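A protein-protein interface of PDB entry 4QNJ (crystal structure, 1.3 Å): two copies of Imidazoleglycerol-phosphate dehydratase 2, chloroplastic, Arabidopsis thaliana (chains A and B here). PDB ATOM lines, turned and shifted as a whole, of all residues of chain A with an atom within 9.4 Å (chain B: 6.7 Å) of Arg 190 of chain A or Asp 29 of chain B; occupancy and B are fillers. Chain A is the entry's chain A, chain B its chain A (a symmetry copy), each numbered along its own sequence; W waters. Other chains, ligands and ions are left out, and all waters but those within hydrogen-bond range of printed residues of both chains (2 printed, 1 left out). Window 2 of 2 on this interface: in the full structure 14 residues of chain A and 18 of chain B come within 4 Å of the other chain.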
ATOM      1  N   GLY A  94       8.747 -33.382 -26.373  1.00  0.00           N
ATOM      2  CA  GLY A  94       8.612 -32.730 -25.068  1.00  0.00           C
ATOM      3  C   GLY A  94       9.892 -32.287 -24.388  1.00  0.00           C
ATOM      4  O   GLY A  94       9.851 -31.867 -23.242  1.00  0.00           O
ATOM      5  N   ILE A  95      11.012 -32.356 -25.094  1.00  0.00           N
ATOM      6  CA  ILE A  95      12.306 -32.033 -24.494  1.00  0.00           C
ATOM      7  C   ILE A  95      12.631 -30.551 -24.621  1.00  0.00           C
ATOM      8  O   ILE A  95      12.095 -29.845 -25.472  1.00  0.00           O
ATOM      9  CB  ILE A  95      13.461 -32.897 -25.035  1.00  0.00           C
ATOM     10  CG1 ILE A  95      13.760 -32.582 -26.510  1.00  0.00           C
ATOM     11  CG2 ILE A  95      13.157 -34.364 -24.755  1.00  0.00           C
ATOM     12  CD1 ILE A  95      15.023 -33.240 -27.038  1.00  0.00           C
ATOM     13  N   ASN A  96      13.506 -30.081 -23.747  1.00  0.00           N
ATOM     14  CA  ASN A  96      13.981 -28.690 -23.835  1.00  0.00           C
ATOM     15  C   ASN A  96      14.643 -28.384 -25.194  1.00  0.00           C
ATOM     16  O   ASN A  96      14.490 -27.288 -25.728  1.00  0.00           O
ATOM     17  CB  ASN A  96      14.958 -28.362 -22.703  1.00  0.00           C
ATOM     18  CG  ASN A  96      14.272 -28.174 -21.351  1.00  0.00           C
ATOM     19  OD1 ASN A  96      13.210 -27.546 -21.250  1.00  0.00           O
ATOM     20  ND2 ASN A  96      14.886 -28.717 -20.299  1.00  0.00           N
ATOM     21  N   GLU A 186      16.430 -33.073 -21.038  1.00  0.00           N
ATOM     22  CA  GLU A 186      15.362 -33.097 -20.028  1.00  0.00           C
ATOM     23  C   GLU A 186      14.047 -32.574 -20.598  1.00  0.00           C
ATOM     24  O   GLU A 186      13.995 -31.865 -21.602  1.00  0.00           O
ATOM     25  CB  GLU A 186      15.739 -32.320 -18.757  1.00  0.00           C
ATOM     26  CG  GLU A 186      16.696 -33.092 -17.862  1.00  0.00           C
ATOM     27  CD  GLU A 186      17.182 -32.318 -16.656  1.00  0.00           C
ATOM     28  OE1 GLU A 186      17.114 -31.078 -16.661  1.00  0.00           O
ATOM     29  OE2 GLU A 186      17.670 -32.964 -15.701  1.00  0.00           O
ATOM     30  N   SER A 187      12.982 -32.954 -19.918  1.00  0.00           N
ATOM     31  CA  SER A 187      11.645 -32.564 -20.296  1.00  0.00           C
ATOM     32  C   SER A 187      11.430 -31.059 -20.054  1.00  0.00           C
ATOM     33  O   SER A 187      11.878 -30.495 -19.060  1.00  0.00           O
ATOM     34  CB  SER A 187      10.641 -33.424 -19.528  1.00  0.00           C
ATOM     35  OG  SER A 187      10.673 -33.128 -18.147  1.00  0.00           O
ATOM     36  N   ASP A 188      10.764 -30.425 -21.003  1.00  0.00           N
ATOM     37  CA  ASP A 188      10.295 -29.047 -20.847  1.00  0.00           C
ATOM     38  C   ASP A 188       8.914 -29.161 -20.192  1.00  0.00           C
ATOM     39  O   ASP A 188       8.006 -29.735 -20.792  1.00  0.00           O
ATOM     40  CB  ASP A 188      10.213 -28.371 -22.218  1.00  0.00           C
ATOM     41  CG  ASP A 188       9.759 -26.929 -22.144  1.00  0.00           C
ATOM     42  OD1 ASP A 188       8.919 -26.600 -21.272  1.00  0.00           O
ATOM     43  OD2 ASP A 188      10.232 -26.116 -22.968  1.00  0.00           O
ATOM     44  N   PRO A 189       8.744 -28.628 -18.967  1.00  0.00           N
ATOM     45  CA  PRO A 189       7.489 -28.801 -18.229  1.00  0.00           C
ATOM     46  C   PRO A 189       6.261 -28.194 -18.910  1.00  0.00           C
ATOM     47  O   PRO A 189       5.136 -28.555 -18.566  1.00  0.00           O
ATOM     48  CB  PRO A 189       7.770 -28.081 -16.907  1.00  0.00           C
ATOM     49  CG  PRO A 189       8.771 -27.041 -17.267  1.00  0.00           C
ATOM     50  CD  PRO A 189       9.666 -27.729 -18.256  1.00  0.00           C
ATOM     51  N   ARG A 190       6.472 -27.281 -19.852  1.00  0.00           N
ATOM     52  CA  ARG A 190       5.343 -26.683 -20.613  1.00  0.00           C
ATOM     53  C   ARG A 190       5.136 -27.267 -22.012  1.00  0.00           C
ATOM     54  O   ARG A 190       4.304 -26.781 -22.781  1.00  0.00           O
ATOM     55  CB  ARG A 190       5.486 -25.167 -20.688  1.00  0.00           C
ATOM     56  CG  ARG A 190       5.212 -24.502 -19.344  1.00  0.00           C
ATOM     57  CD  ARG A 190       5.509 -23.019 -19.346  1.00  0.00           C
ATOM     58  NE  ARG A 190       4.560 -22.312 -20.208  1.00  0.00           N
ATOM     59  CZ  ARG A 190       4.710 -21.059 -20.624  1.00  0.00           C
ATOM     60  NH1 ARG A 190       5.778 -20.382 -20.256  1.00  0.00           N
ATOM     61  NH2 ARG A 190       3.807 -20.484 -21.408  1.00  0.00           N
ATOM     62  N   ARG A 191       5.865 -28.327 -22.331  1.00  0.00           N
ATOM     63  CA  ARG A 191       5.746 -28.955 -23.658  1.00  0.00           C
ATOM     64  C   ARG A 191       5.242 -30.392 -23.550  1.00  0.00           C
ATOM     65  O   ARG A 191       5.407 -31.177 -24.483  1.00  0.00           O
ATOM     66  CB  ARG A 191       7.075 -28.906 -24.429  1.00  0.00           C
ATOM     67  CG  ARG A 191       7.491 -27.499 -24.850  1.00  0.00           C
ATOM     68  CD  ARG A 191       8.803 -27.472 -25.627  1.00  0.00           C
ATOM     69  NE  ARG A 191       9.283 -26.100 -25.821  1.00  0.00           N
ATOM     70  CZ  ARG A 191       8.863 -25.261 -26.773  1.00  0.00           C
ATOM     71  NH1 ARG A 191       7.966 -25.649 -27.675  1.00  0.00           N
ATOM     72  NH2 ARG A 191       9.376 -24.032 -26.842  1.00  0.00           N
ATOM     73  N   ALA B   8      -4.688 -16.491 -17.087  1.00  0.00           N
ATOM     74  CA  ALA B   8      -3.643 -16.140 -18.106  1.00  0.00           C
ATOM     75  C   ALA B   8      -3.486 -14.630 -18.243  1.00  0.00           C
ATOM     76  O   ALA B   8      -4.460 -13.879 -18.234  1.00  0.00           O
ATOM     77  CB  ALA B   8      -3.970 -16.754 -19.466  1.00  0.00           C
ATOM     78  N   ARG B   9      -2.240 -14.215 -18.402  1.00  0.00           N
ATOM     79  CA  ARG B   9      -1.872 -12.795 -18.539  1.00  0.00           C
ATOM     80  C   ARG B   9      -1.856 -12.364 -20.001  1.00  0.00           C
ATOM     81  O   ARG B   9      -0.948 -12.701 -20.762  1.00  0.00           O
ATOM     82  CB  ARG B   9      -0.511 -12.562 -17.912  1.00  0.00           C
ATOM     83  CG  ARG B   9      -0.521 -12.636 -16.395  1.00  0.00           C
ATOM     84  CD  ARG B   9       0.897 -12.691 -15.867  1.00  0.00           C
ATOM     85  NE  ARG B   9       1.595 -13.865 -16.396  1.00  0.00           N
ATOM     86  CZ  ARG B   9       2.915 -14.039 -16.378  1.00  0.00           C
ATOM     87  NH1 ARG B   9       3.721 -13.112 -15.862  1.00  0.00           N
ATOM     88  NH2 ARG B   9       3.428 -15.149 -16.884  1.00  0.00           N
ATOM     89  N   ILE B  10      -2.899 -11.639 -20.386  1.00  0.00           N
ATOM     90  CA  ILE B  10      -3.120 -11.222 -21.776  1.00  0.00           C
ATOM     91  C   ILE B  10      -3.075  -9.705 -21.891  1.00  0.00           C
ATOM     92  O   ILE B  10      -3.732  -8.980 -21.131  1.00  0.00           O
ATOM     93  CB  ILE B  10      -4.453 -11.775 -22.317  1.00  0.00           C
ATOM     94  CG1 ILE B  10      -4.379 -13.309 -22.301  1.00  0.00           C
ATOM     95  CG2 ILE B  10      -4.748 -11.247 -23.720  1.00  0.00           C
ATOM     96  CD1 ILE B  10      -5.689 -14.023 -22.550  1.00  0.00           C
ATOM     97  N   ILE B  26      -1.052 -10.499 -26.921  1.00  0.00           N
ATOM     98  CA  ILE B  26      -0.067 -11.475 -26.431  1.00  0.00           C
ATOM     99  C   ILE B  26      -0.522 -12.104 -25.128  1.00  0.00           C
ATOM    100  O   ILE B  26      -0.954 -11.404 -24.202  1.00  0.00           O
ATOM    101  CB  ILE B  26       1.326 -10.836 -26.272  1.00  0.00           C
ATOM    102  CG1 ILE B  26       1.777 -10.345 -27.646  1.00  0.00           C
ATOM    103  CG2 ILE B  26       2.353 -11.829 -25.730  1.00  0.00           C
ATOM    104  CD1 ILE B  26       3.096  -9.623 -27.650  1.00  0.00           C
ATOM    105  N   ASN B  27      -0.423 -13.425 -25.072  1.00  0.00           N
ATOM    106  CA  ASN B  27      -0.652 -14.201 -23.838  1.00  0.00           C
ATOM    107  C   ASN B  27       0.705 -14.673 -23.321  1.00  0.00           C
ATOM    108  O   ASN B  27       1.390 -15.447 -23.987  1.00  0.00           O
ATOM    109  CB  ASN B  27      -1.553 -15.395 -24.120  1.00  0.00           C
ATOM    110  CG  ASN B  27      -1.941 -16.172 -22.876  1.00  0.00           C
ATOM    111  OD1 ASN B  27      -1.384 -16.016 -21.796  1.00  0.00           O
ATOM    112  ND2 ASN B  27      -2.935 -17.018 -23.038  1.00  0.00           N
ATOM    113  N   LEU B  28       1.081 -14.193 -22.142  1.00  0.00           N
ATOM    114  CA  LEU B  28       2.369 -14.585 -21.523  1.00  0.00           C
ATOM    115  C   LEU B  28       2.397 -16.031 -21.070  1.00  0.00           C
ATOM    116  O   LEU B  28       3.457 -16.643 -20.930  1.00  0.00           O
ATOM    117  CB  LEU B  28       2.723 -13.701 -20.338  1.00  0.00           C
ATOM    118  CG  LEU B  28       2.809 -12.213 -20.632  1.00  0.00           C
ATOM    119  CD1 LEU B  28       3.209 -11.476 -19.364  1.00  0.00           C
ATOM    120  CD2 LEU B  28       3.808 -11.938 -21.744  1.00  0.00           C
ATOM    121  N   ASP B  29       1.198 -16.559 -20.850  1.00  0.00           N
ATOM    122  CA  ASP B  29       1.003 -17.927 -20.349  1.00  0.00           C
ATOM    123  C   ASP B  29       0.417 -18.828 -21.435  1.00  0.00           C
ATOM    124  O   ASP B  29      -0.502 -19.618 -21.209  1.00  0.00           O
ATOM    125  CB  ASP B  29       0.118 -17.895 -19.112  1.00  0.00           C
ATOM    126  CG  ASP B  29       0.658 -16.978 -18.050  1.00  0.00           C
ATOM    127  OD1 ASP B  29       1.748 -17.291 -17.527  1.00  0.00           O
ATOM    128  OD2 ASP B  29       0.009 -15.945 -17.758  1.00  0.00           O
ATOM    129  N   GLY B  30       0.999 -18.709 -22.613  1.00  0.00           N
ATOM    130  CA  GLY B  30       0.473 -19.359 -23.805  1.00  0.00           C
ATOM    131  C   GLY B  30       0.996 -20.755 -24.073  1.00  0.00           C
ATOM    132  O   GLY B  30       1.639 -21.398 -23.236  1.00  0.00           O
ATOM    133  N   HIS B  31       0.696 -21.194 -25.286  1.00  0.00           N
ATOM    134  CA  HIS B  31       1.117 -22.503 -25.807  1.00  0.00           C
ATOM    135  C   HIS B  31       1.847 -22.377 -27.128  1.00  0.00           C
ATOM    136  O   HIS B  31       2.024 -23.355 -27.844  1.00  0.00           O
ATOM    137  CB  HIS B  31      -0.068 -23.445 -25.980  1.00  0.00           C
ATOM    138  CG  HIS B  31      -0.767 -23.746 -24.699  1.00  0.00           C
ATOM    139  ND1 HIS B  31      -1.689 -22.888 -24.142  1.00  0.00           N
ATOM    140  CD2 HIS B  31      -0.638 -24.778 -23.834  1.00  0.00           C
ATOM    141  CE1 HIS B  31      -2.127 -23.397 -23.006  1.00  0.00           C
ATOM    142  NE2 HIS B  31      -1.505 -24.543 -22.794  1.00  0.00           N
ATOM    143  N   GLY B  32       2.299 -21.175 -27.442  1.00  0.00           N
ATOM    144  CA  GLY B  32       3.024 -20.988 -28.693  1.00  0.00           C
ATOM    145  C   GLY B  32       2.165 -20.798 -29.931  1.00  0.00           C
ATOM    146  O   GLY B  32       2.633 -21.024 -31.047  1.00  0.00           O
ATOM    147  N   GLY B  54       9.123 -18.983 -27.169  1.00  0.00           N
ATOM    148  CA  GLY B  54       8.750 -18.369 -25.895  1.00  0.00           C
ATOM    149  C   GLY B  54       7.537 -18.975 -25.223  1.00  0.00           C
ATOM    150  O   GLY B  54       7.270 -18.680 -24.066  1.00  0.00           O
ATOM    151  N   LEU B  55       6.796 -19.804 -25.959  1.00  0.00           N
ATOM    152  CA  LEU B  55       5.475 -20.307 -25.544  1.00  0.00           C
ATOM    153  C   LEU B  55       4.522 -19.163 -25.212  1.00  0.00           C
ATOM    154  O   LEU B  55       3.694 -19.254 -24.315  1.00  0.00           O
ATOM    155  CB  LEU B  55       5.605 -21.319 -24.398  1.00  0.00           C
ATOM    156  CG  LEU B  55       6.342 -22.613 -24.813  1.00  0.00           C
ATOM    157  CD1 LEU B  55       6.332 -23.600 -23.653  1.00  0.00           C
ATOM    158  CD2 LEU B  55       5.735 -23.262 -26.053  1.00  0.00           C
ATOM    159  N   PHE B  56       4.664 -18.083 -25.960  1.00  0.00           N
ATOM    160  CA  PHE B  56       3.687 -17.011 -25.973  1.00  0.00           C
ATOM    161  C   PHE B  56       2.639 -17.319 -27.029  1.00  0.00           C
ATOM    162  O   PHE B  56       2.943 -17.957 -28.029  1.00  0.00           O
ATOM    163  CB  PHE B  56       4.353 -15.666 -26.279  1.00  0.00           C
ATOM    164  CG  PHE B  56       5.453 -15.331 -25.326  1.00  0.00           C
ATOM    165  CD1 PHE B  56       6.772 -15.214 -25.740  1.00  0.00           C
ATOM    166  CD2 PHE B  56       5.166 -15.188 -23.987  1.00  0.00           C
ATOM    167  CE1 PHE B  56       7.775 -14.929 -24.824  1.00  0.00           C
ATOM    168  CE2 PHE B  56       6.157 -14.905 -23.069  1.00  0.00           C
ATOM    169  CZ  PHE B  56       7.463 -14.769 -23.490  1.00  0.00           C
ATOM    170  N   ASP B  57       1.409 -16.875 -26.797  1.00  0.00           N
ATOM    171  CA  ASP B  57       0.437 -16.781 -27.894  1.00  0.00           C
ATOM    172  C   ASP B  57       0.546 -15.368 -28.435  1.00  0.00           C
ATOM    173  O   ASP B  57       0.454 -14.392 -27.698  1.00  0.00           O
ATOM    174  CB  ASP B  57      -1.004 -17.107 -27.498  1.00  0.00           C
ATOM    175  CG  ASP B  57      -1.169 -18.531 -26.985  1.00  0.00           C
ATOM    176  OD1 ASP B  57      -0.321 -19.412 -27.265  1.00  0.00           O
ATOM    177  OD2 ASP B  57      -2.176 -18.766 -26.284  1.00  0.00           O
ATOM    178  N   ALA B  88       0.183  -6.881 -20.194  1.00  0.00           N
ATOM    179  CA  ALA B  88       0.071  -8.290 -19.773  1.00  0.00           C
ATOM    180  C   ALA B  88       0.770  -8.540 -18.437  1.00  0.00           C
ATOM    181  O   ALA B  88       0.306  -9.326 -17.609  1.00  0.00           O
ATOM    182  CB  ALA B  88       0.623  -9.233 -20.829  1.00  0.00           C
ATOM    183  N   ARG B 182      10.572 -15.667 -21.871  1.00  0.00           N
ATOM    184  CA  ARG B 182       9.807 -16.733 -21.199  1.00  0.00           C
ATOM    185  C   ARG B 182      10.285 -16.863 -19.754  1.00  0.00           C
ATOM    186  O   ARG B 182       9.487 -16.847 -18.808  1.00  0.00           O
ATOM    187  CB  ARG B 182       9.933 -18.075 -21.932  1.00  0.00           C
ATOM    188  CG  ARG B 182       9.410 -19.259 -21.139  1.00  0.00           C
ATOM    189  CD  ARG B 182       9.469 -20.562 -21.920  1.00  0.00           C
ATOM    190  NE  ARG B 182       9.154 -21.671 -21.023  1.00  0.00           N
ATOM    191  CZ  ARG B 182       9.225 -22.960 -21.333  1.00  0.00           C
ATOM    192  NH1 ARG B 182       9.583 -23.348 -22.545  1.00  0.00           N
ATOM    193  NH2 ARG B 182       8.940 -23.872 -20.414  1.00  0.00           N
ATOM    194  N   THR B 185       9.324 -13.785 -17.542  1.00  0.00           N
ATOM    195  CA  THR B 185       7.873 -13.653 -17.309  1.00  0.00           C
ATOM    196  C   THR B 185       7.268 -14.789 -16.478  1.00  0.00           C
ATOM    197  O   THR B 185       6.175 -14.636 -15.929  1.00  0.00           O
ATOM    198  CB  THR B 185       7.065 -13.542 -18.616  1.00  0.00           C
ATOM    199  OG1 THR B 185       7.245 -14.718 -19.422  1.00  0.00           O
ATOM    200  CG2 THR B 185       7.442 -12.287 -19.365  1.00  0.00           C
ATOM    201  N   GLU B 186       7.972 -15.913 -16.386  1.00  0.00           N
ATOM    202  CA  GLU B 186       7.513 -17.061 -15.591  1.00  0.00           C
ATOM    203  C   GLU B 186       7.616 -16.778 -14.096  1.00  0.00           C
ATOM    204  O   GLU B 186       8.349 -15.904 -13.635  1.00  0.00           O
ATOM    205  CB  GLU B 186       8.263 -18.355 -15.943  1.00  0.00           C
ATOM    206  CG  GLU B 186       7.780 -18.975 -17.245  1.00  0.00           C
ATOM    207  CD  GLU B 186       8.568 -20.188 -17.687  1.00  0.00           C
ATOM    208  OE1 GLU B 186       9.712 -20.368 -17.237  1.00  0.00           O
ATOM    209  OE2 GLU B 186       8.043 -20.957 -18.525  1.00  0.00           O
ATOM    210  N   SER B 187       6.851 -17.554 -13.352  1.00  0.00           N
ATOM    211  CA  SER B 187       6.807 -17.444 -11.913  1.00  0.00           C
ATOM    212  C   SER B 187       8.130 -17.925 -11.292  1.00  0.00           C
ATOM    213  O   SER B 187       8.727 -18.907 -11.723  1.00  0.00           O
ATOM    214  CB  SER B 187       5.602 -18.229 -11.393  1.00  0.00           C
ATOM    215  OG  SER B 187       5.777 -19.617 -11.594  1.00  0.00           O
HETATM  216  O   HOH W   1       1.949 -23.414 -21.020  1.00  0.00           O
HETATM  217  O   HOH W   2      10.896 -22.492 -24.828  1.00  0.00           O
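O of Gly 30 of chain B lies within hydrogen-bond range of NH2 of Arg 190 of chain A. NH2 of Arg 182 of chain B is in salt-bridge range of OD1 of Asp 188 of chain A (2.9 Å). OE2 of Glu 186 of chain B is in salt-bridge range of NH1 of Arg 190 of chain A (2.9 Å). NH2 of Arg 190 of chain A lies within hydrogen-bond range of O of Leu 55 of chain B.
The guanidinium group (NE) of Arg 182 of chain B lies within salt-bridge range of the side-chain carboxylate (OE2) of Glu 186 of chain B (2.8 Å). O of Arg 182 of chain B is in hydrogen-bond range of OG1 of Thr 185 of chain B (3.2 Å). OD1 of Asp 188 of chain A lies within hydrogen-bond range of N of Arg 190 of chain A, 2.9 Å away. The backbone carbonyl oxygen (O) of Gly 94 of chain A sits at hydrogen-bond distance from the backbone NH (N) of Asp 188 of chain A, at 2.8 Å. The backbone carbonyl oxygen (O) of Arg 9 of chain B lies within hydrogen-bond range of the backbone NH (N) of Leu 28 of chain B (2.9 Å). The side-chain carboxylate (OD2) of Asp 188 of chain A lies within salt-bridge range of the guanidinium group (NE) of Arg 191 of chain A (3.0 Å).
Arg 190 of chain A touches Leu 28 of chain B. Arg 190 of chain A touches Asp 29 of chain B (NH2 to C, 3.8 Å). CD of Arg 190 of chain A touches NH2 of Arg 182 of chain B, at 3.7 Å. CD2 of Leu 55 of chain B touches NH1 of Arg 191 of chain A, 3.6 Å away.
Arg 190 of chain A touches just these residues of chain B: Leu 28, Asp 29, Gly 30, Leu 55, Arg 182 and Glu 186. Of the printed residues of chain B, Arg 191 of chain A touches Leu 55. Ala 8 of chain B touches none of the printed residues of chain A. Of the printed residues of chain A, Gly 30 of chain B touches Arg 190. Printed residues of chain A within 4 Å of Leu 55 of chain B: Arg 190 (3.2 Å) and Arg 191 (3.6 Å). Of the printed residues of chain A, Arg 182 of chain B touches Asp 188 and Arg 190. The nearest residue of chain B that does not touch Arg 190 of chain A is Gly 54 of chain B (4.4 Å).
Printed residues of chain A that touch a printed residue of chain B: Asp 188, Arg 190 and Arg 191. Among the printed residues, 8 pairs touch across the chains. Among the printed residues, Asp or Glu carboxylates within 4 Å of a Lys or Arg side-chain nitrogen of the other chain: Asp 188 of chain A with Arg 182 of chain B (2.9 Å) and Arg 190 of chain A with Glu 186 of chain B (2.9 Å).
Positions printed for both chains: 186 and 187. Of the 8 pairs that touch across the chains among the printed residues, none has its exchanged pair printed and touching as well.
Water W2 bridges NH1 of Arg 182 of chain B and NH2 of Arg 191 of chain A. Water W1 lies within hydrogen-bond range of the guanidinium group (NE) of Arg 190 of chain A (2.9 Å) and the backbone carbonyl oxygen (O) of Gly 30 of chain B (3.0 Å).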
